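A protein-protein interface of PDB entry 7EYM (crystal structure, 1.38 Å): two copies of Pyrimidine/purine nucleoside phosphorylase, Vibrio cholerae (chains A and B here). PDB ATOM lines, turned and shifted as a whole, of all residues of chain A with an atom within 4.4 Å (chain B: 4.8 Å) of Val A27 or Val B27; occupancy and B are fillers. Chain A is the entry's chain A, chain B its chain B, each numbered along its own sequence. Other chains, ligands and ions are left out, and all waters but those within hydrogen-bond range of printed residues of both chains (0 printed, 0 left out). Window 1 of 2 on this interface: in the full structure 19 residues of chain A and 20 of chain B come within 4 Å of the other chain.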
ATOM      1  N   SER A  15      24.433  14.246  -6.621  1.00  0.00           N
ATOM      2  CA  SER A  15      23.872  15.207  -5.684  1.00  0.00           C
ATOM      3  C   SER A  15      24.584  15.113  -4.345  1.00  0.00           C
ATOM      4  O   SER A  15      25.203  14.093  -4.013  1.00  0.00           O
ATOM      5  CB  SER A  15      22.355  15.059  -5.518  1.00  0.00           C
ATOM      6  OG  SER A  15      22.022  13.879  -4.819  1.00  0.00           O
ATOM      7  N   LEU A  16      24.508  16.213  -3.597  1.00  0.00           N
ATOM      8  CA  LEU A  16      25.042  16.319  -2.245  1.00  0.00           C
ATOM      9  C   LEU A  16      23.918  16.720  -1.301  1.00  0.00           C
ATOM     10  O   LEU A  16      23.329  17.801  -1.451  1.00  0.00           O
ATOM     11  CB  LEU A  16      26.155  17.360  -2.220  1.00  0.00           C
ATOM     12  CG  LEU A  16      27.357  17.099  -3.138  1.00  0.00           C
ATOM     13  CD1 LEU A  16      28.242  18.329  -3.187  1.00  0.00           C
ATOM     14  CD2 LEU A  16      28.147  15.876  -2.679  1.00  0.00           C
ATOM     15  N   PHE A  18      22.517  17.747   2.408  1.00  0.00           N
ATOM     16  CA  PHE A  18      23.031  18.461   3.562  1.00  0.00           C
ATOM     17  C   PHE A  18      21.864  18.874   4.441  1.00  0.00           C
ATOM     18  O   PHE A  18      20.763  19.142   3.958  1.00  0.00           O
ATOM     19  CB  PHE A  18      23.892  19.676   3.157  1.00  0.00           C
ATOM     20  CG  PHE A  18      23.159  20.723   2.343  1.00  0.00           C
ATOM     21  CD1 PHE A  18      22.913  20.527   0.984  1.00  0.00           C
ATOM     22  CD2 PHE A  18      22.722  21.906   2.934  1.00  0.00           C
ATOM     23  CE1 PHE A  18      22.241  21.493   0.236  1.00  0.00           C
ATOM     24  CE2 PHE A  18      22.050  22.882   2.194  1.00  0.00           C
ATOM     25  CZ  PHE A  18      21.810  22.674   0.834  1.00  0.00           C
ATOM     26  N   THR A  26      19.210  19.277  -1.014  1.00  0.00           N
ATOM     27  CA  THR A  26      20.266  18.733  -1.858  1.00  0.00           C
ATOM     28  C   THR A  26      20.643  19.729  -2.935  1.00  0.00           C
ATOM     29  O   THR A  26      19.799  20.476  -3.442  1.00  0.00           O
ATOM     30  CB  THR A  26      19.895  17.397  -2.531  1.00  0.00           C
ATOM     31  OG1 THR A  26      18.927  17.618  -3.563  1.00  0.00           O
ATOM     32  CG2 THR A  26      19.348  16.412  -1.522  1.00  0.00           C
ATOM     33  N   VAL A  27      21.929  19.755  -3.290  1.00  0.00           N
ATOM     34  CA  VAL A  27      22.402  20.461  -4.477  1.00  0.00           C
ATOM     35  C   VAL A  27      23.062  19.438  -5.393  1.00  0.00           C
ATOM     36  O   VAL A  27      23.785  18.556  -4.922  1.00  0.00           O
ATOM     37  CB  VAL A  27      23.354  21.627  -4.107  1.00  0.00           C
ATOM     38  CG1 VAL A  27      24.663  21.121  -3.492  1.00  0.00           C
ATOM     39  CG2 VAL A  27      23.622  22.546  -5.286  1.00  0.00           C
ATOM     40  N   GLY A  28      22.787  19.524  -6.696  1.00  0.00           N
ATOM     41  CA  GLY A  28      23.266  18.499  -7.594  1.00  0.00           C
ATOM     42  C   GLY A  28      23.570  19.019  -8.975  1.00  0.00           C
ATOM     43  O   GLY A  28      23.375  20.195  -9.282  1.00  0.00           O
ATOM     44  N   VAL A  29      24.054  18.104  -9.813  1.00  0.00           N
ATOM     45  CA  VAL A  29      24.364  18.387 -11.205  1.00  0.00           C
ATOM     46  C   VAL A  29      23.787  17.274 -12.063  1.00  0.00           C
ATOM     47  O   VAL A  29      23.896  16.092 -11.716  1.00  0.00           O
ATOM     48  CB  VAL A  29      25.883  18.513 -11.442  1.00  0.00           C
ATOM     49  CG1 VAL A  29      26.183  18.723 -12.931  1.00  0.00           C
ATOM     50  CG2 VAL A  29      26.488  19.631 -10.601  1.00  0.00           C
ATOM     51  N   VAL A  48      20.203  26.398 -10.592  1.00  0.00           N
ATOM     52  CA  VAL A  48      21.319  27.229 -10.139  1.00  0.00           C
ATOM     53  C   VAL A  48      22.149  27.744 -11.307  1.00  0.00           C
ATOM     54  O   VAL A  48      22.501  28.927 -11.352  1.00  0.00           O
ATOM     55  CB  VAL A  48      22.172  26.433  -9.129  1.00  0.00           C
ATOM     56  CG1 VAL A  48      23.477  27.190  -8.818  1.00  0.00           C
ATOM     57  CG2 VAL A  48      21.358  26.148  -7.854  1.00  0.00           C
ATOM     58  N   ALA A  88      23.364  22.677 -12.776  1.00  0.00           N
ATOM     59  CA  ALA A  88      23.313  22.569 -11.326  1.00  0.00           C
ATOM     60  C   ALA A  88      21.944  23.001 -10.817  1.00  0.00           C
ATOM     61  O   ALA A  88      21.316  23.911 -11.370  1.00  0.00           O
ATOM     62  CB  ALA A  88      24.369  23.464 -10.693  1.00  0.00           C
ATOM     63  N   TYR A  89      21.484  22.345  -9.751  1.00  0.00           N
ATOM     64  CA  TYR A  89      20.155  22.576  -9.203  1.00  0.00           C
ATOM     65  C   TYR A  89      20.192  22.468  -7.683  1.00  0.00           C
ATOM     66  O   TYR A  89      21.085  21.841  -7.104  1.00  0.00           O
ATOM     67  CB  TYR A  89      19.124  21.585  -9.783  1.00  0.00           C
ATOM     68  CG  TYR A  89      19.399  20.150  -9.386  1.00  0.00           C
ATOM     69  CD1 TYR A  89      20.251  19.338 -10.143  1.00  0.00           C
ATOM     70  CD2 TYR A  89      18.857  19.616  -8.216  1.00  0.00           C
ATOM     71  CE1 TYR A  89      20.518  18.024  -9.759  1.00  0.00           C
ATOM     72  CE2 TYR A  89      19.121  18.303  -7.825  1.00  0.00           C
ATOM     73  CZ  TYR A  89      19.961  17.515  -8.601  1.00  0.00           C
ATOM     74  OH  TYR A  89      20.251  16.211  -8.245  1.00  0.00           O
ATOM     75  N   LYS B  14      32.435  19.159   0.149  1.00  0.00           N
ATOM     76  CA  LYS B  14      32.342  18.346  -1.054  1.00  0.00           C
ATOM     77  C   LYS B  14      31.833  19.213  -2.191  1.00  0.00           C
ATOM     78  O   LYS B  14      31.029  20.126  -1.981  1.00  0.00           O
ATOM     79  CB  LYS B  14      31.422  17.143  -0.880  1.00  0.00           C
ATOM     80  CG  LYS B  14      31.836  16.206   0.253  1.00  0.00           C
ATOM     81  CD  LYS B  14      31.021  14.922   0.286  1.00  0.00           C
ATOM     82  CE  LYS B  14      31.532  13.989   1.375  1.00  0.00           C
ATOM     83  NZ  LYS B  14      30.686  12.750   1.429  1.00  0.00           N
ATOM     84  N   SER B  15      32.325  18.934  -3.395  1.00  0.00           N
ATOM     85  CA  SER B  15      31.974  19.727  -4.562  1.00  0.00           C
ATOM     86  C   SER B  15      31.769  18.821  -5.762  1.00  0.00           C
ATOM     87  O   SER B  15      32.298  17.707  -5.819  1.00  0.00           O
ATOM     88  CB  SER B  15      33.022  20.804  -4.852  1.00  0.00           C
ATOM     89  OG  SER B  15      34.223  20.239  -5.358  1.00  0.00           O
ATOM     90  N   LEU B  16      30.980  19.317  -6.713  1.00  0.00           N
ATOM     91  CA  LEU B  16      30.705  18.661  -7.984  1.00  0.00           C
ATOM     92  C   LEU B  16      31.104  19.625  -9.089  1.00  0.00           C
ATOM     93  O   LEU B  16      30.528  20.714  -9.204  1.00  0.00           O
ATOM     94  CB  LEU B  16      29.223  18.294  -8.101  1.00  0.00           C
ATOM     95  CG  LEU B  16      28.706  17.318  -7.046  1.00  0.00           C
ATOM     96  CD1 LEU B  16      27.195  17.206  -7.086  1.00  0.00           C
ATOM     97  CD2 LEU B  16      29.341  15.947  -7.226  1.00  0.00           C
ATOM     98  N   PHE B  18      31.547  20.590 -13.099  1.00  0.00           N
ATOM     99  CA  PHE B  18      30.857  20.326 -14.350  1.00  0.00           C
ATOM    100  C   PHE B  18      31.277  21.366 -15.379  1.00  0.00           C
ATOM    101  O   PHE B  18      31.695  22.470 -15.027  1.00  0.00           O
ATOM    102  CB  PHE B  18      29.327  20.302 -14.167  1.00  0.00           C
ATOM    103  CG  PHE B  18      28.743  21.582 -13.634  1.00  0.00           C
ATOM    104  CD1 PHE B  18      28.831  21.898 -12.285  1.00  0.00           C
ATOM    105  CD2 PHE B  18      28.092  22.470 -14.479  1.00  0.00           C
ATOM    106  CE1 PHE B  18      28.278  23.074 -11.798  1.00  0.00           C
ATOM    107  CE2 PHE B  18      27.538  23.648 -13.994  1.00  0.00           C
ATOM    108  CZ  PHE B  18      27.640  23.954 -12.646  1.00  0.00           C
ATOM    109  N   SER B  25      32.518  24.923 -13.882  1.00  0.00           N
ATOM    110  CA  SER B  25      31.969  25.563 -12.695  1.00  0.00           C
ATOM    111  C   SER B  25      31.856  24.469 -11.658  1.00  0.00           C
ATOM    112  O   SER B  25      31.987  23.280 -11.964  1.00  0.00           O
ATOM    113  CB  SER B  25      30.576  26.132 -12.977  1.00  0.00           C
ATOM    114  OG  SER B  25      30.641  27.218 -13.880  1.00  0.00           O
ATOM    115  N   THR B  26      31.644  24.844 -10.399  1.00  0.00           N
ATOM    116  CA  THR B  26      31.360  23.835  -9.380  1.00  0.00           C
ATOM    117  C   THR B  26      30.183  24.254  -8.516  1.00  0.00           C
ATOM    118  O   THR B  26      29.933  25.443  -8.310  1.00  0.00           O
ATOM    119  CB  THR B  26      32.555  23.499  -8.443  1.00  0.00           C
ATOM    120  OG1 THR B  26      32.934  24.651  -7.677  1.00  0.00           O
ATOM    121  CG2 THR B  26      33.748  22.989  -9.230  1.00  0.00           C
ATOM    122  N   VAL B  27      29.460  23.261  -8.011  1.00  0.00           N
ATOM    123  CA  VAL B  27      28.567  23.471  -6.881  1.00  0.00           C
ATOM    124  C   VAL B  27      29.080  22.609  -5.746  1.00  0.00           C
ATOM    125  O   VAL B  27      29.727  21.584  -5.970  1.00  0.00           O
ATOM    126  CB  VAL B  27      27.077  23.184  -7.178  1.00  0.00           C
ATOM    127  CG1 VAL B  27      26.504  24.280  -8.056  1.00  0.00           C
ATOM    128  CG2 VAL B  27      26.894  21.809  -7.782  1.00  0.00           C
ATOM    129  N   GLY B  28      28.820  23.038  -4.521  1.00  0.00           N
ATOM    130  CA  GLY B  28      29.309  22.256  -3.408  1.00  0.00           C
ATOM    131  C   GLY B  28      28.594  22.590  -2.124  1.00  0.00           C
ATOM    132  O   GLY B  28      27.677  23.413  -2.087  1.00  0.00           O
ATOM    133  N   VAL B  29      29.013  21.895  -1.072  1.00  0.00           N
ATOM    134  CA  VAL B  29      28.483  22.085   0.266  1.00  0.00           C
ATOM    135  C   VAL B  29      29.647  22.184   1.239  1.00  0.00           C
ATOM    136  O   VAL B  29      30.631  21.439   1.128  1.00  0.00           O
ATOM    137  CB  VAL B  29      27.562  20.918   0.667  1.00  0.00           C
ATOM    138  CG1 VAL B  29      27.095  21.074   2.103  1.00  0.00           C
ATOM    139  CG2 VAL B  29      26.355  20.822  -0.278  1.00  0.00           C
ATOM    140  N   ALA B  88      25.255  25.434   0.873  1.00  0.00           N
ATOM    141  CA  ALA B  88      25.535  25.120  -0.520  1.00  0.00           C
ATOM    142  C   ALA B  88      25.968  26.378  -1.260  1.00  0.00           C
ATOM    143  O   ALA B  88      25.492  27.482  -0.985  1.00  0.00           O
ATOM    144  CB  ALA B  88      24.316  24.496  -1.198  1.00  0.00           C
ATOM    145  N   TYR B  89      26.883  26.208  -2.214  1.00  0.00           N
ATOM    146  CA  TYR B  89      27.465  27.337  -2.924  1.00  0.00           C
ATOM    147  C   TYR B  89      27.678  26.960  -4.385  1.00  0.00           C
ATOM    148  O   TYR B  89      27.771  25.786  -4.742  1.00  0.00           O
ATOM    149  CB  TYR B  89      28.802  27.762  -2.283  1.00  0.00           C
ATOM    150  CG  TYR B  89      29.882  26.706  -2.396  1.00  0.00           C
ATOM    151  CD1 TYR B  89      30.713  26.658  -3.510  1.00  0.00           C
ATOM    152  CD2 TYR B  89      30.057  25.743  -1.406  1.00  0.00           C
ATOM    153  CE1 TYR B  89      31.693  25.686  -3.642  1.00  0.00           C
ATOM    154  CE2 TYR B  89      31.051  24.771  -1.517  1.00  0.00           C
ATOM    155  CZ  TYR B  89      31.860  24.754  -2.645  1.00  0.00           C
ATOM    156  OH  TYR B  89      32.846  23.795  -2.780  1.00  0.00           O
ATOM    157  N   LEU B  90      27.770  27.985  -5.216  1.00  0.00           N
ATOM    158  CA  LEU B  90      28.216  27.879  -6.598  1.00  0.00           C
ATOM    159  C   LEU B  90      29.549  28.604  -6.701  1.00  0.00           C
ATOM    160  O   LEU B  90      29.716  29.693  -6.142  1.00  0.00           O
ATOM    161  CB  LEU B  90      27.179  28.528  -7.527  1.00  0.00           C
ATOM    162  CG  LEU B  90      27.552  28.759  -8.995  1.00  0.00           C
ATOM    163  CD1 LEU B  90      27.597  27.445  -9.738  1.00  0.00           C
ATOM    164  CD2 LEU B  90      26.529  29.690  -9.625  1.00  0.00           C
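The backbone carbonyl oxygen (O) of Phe B18 is in hydrogen-bond range of the backbone NH (N) of Ser B25, at 2.8 Å. N of Val A48 is in hydrogen-bond range of O of Ala A88 (2.8 Å). The backbone carbonyl oxygen of Lys B14 is in hydrogen-bond range of the backbone NH of Val B29 (2.8 Å). O of Val A27 is in hydrogen-bond range of N of Leu A16 (2.8 Å). The backbone NH (N) of Leu B16 lies within hydrogen-bond range of the backbone carbonyl oxygen (O) of Val B27, at 2.7 Å.
Among the printed residues, merely in contact across the chains: Ala A88 with Val B27, Leu A16 with Lys B14, Val A29 with Val B27, Val A27 with Val B29, Phe A18 with Val B29, Val A29 with Phe B18, Phe A18 with Ala B88, Ala A88 with Phe B18, Val A29 with Leu B16, Leu A16 with Leu B16, Leu A16 with Val B29 and Val A27 with Val B27.
Printed residues of chain B within 4 Å of Val A27: Val B27 and Val B29. Printed residues of chain A within 4 Å of Val B27: Val A27 (3.99 Å), Val A29 (3.6 Å) and Ala A88 (3.5 Å). Of the printed residues of chain B, Phe A18 touches Val B29 (3.7 Å) and Ala B88 (3.7 Å). Printed residues of chain B within 4 Å of Ala A88: Phe B18 (3.8 Å) and Val B27 (3.5 Å). Of the printed residues of chain A, Val B29 touches Leu A16 (3.97 Å), Phe A18 (3.7 Å) and Val A27 (3.6 Å). Ser B25 touches none of the printed residues of chain A. Gly A28 touches none of the printed residues of chain B. The nearest printed residue of chain A that does not touch Val B27 is Gly A28 (4.2 Å).
Printed residues of chain B that touch a printed residue of chain A: Lys B14, Leu B16, Phe B18, Val B27, Val B29 and Ala B88. Among the printed residues, no Asp or Glu carboxylate lies within 4 Å of a Lys or Arg side-chain nitrogen of the other chain.
Leu A16 touches Val B29, and with the chains exchanged Val A29 touches Leu B16. Phe A18 touches Val B29, and with the chains exchanged Val A29 touches Phe B18. Phe A18 touches Ala B88, and with the chains exchanged Ala A88 touches Phe B18. Ala A88 touches Val B27, but with the chains exchanged Val A27 does not touch Ala B88 (4.1 Å).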
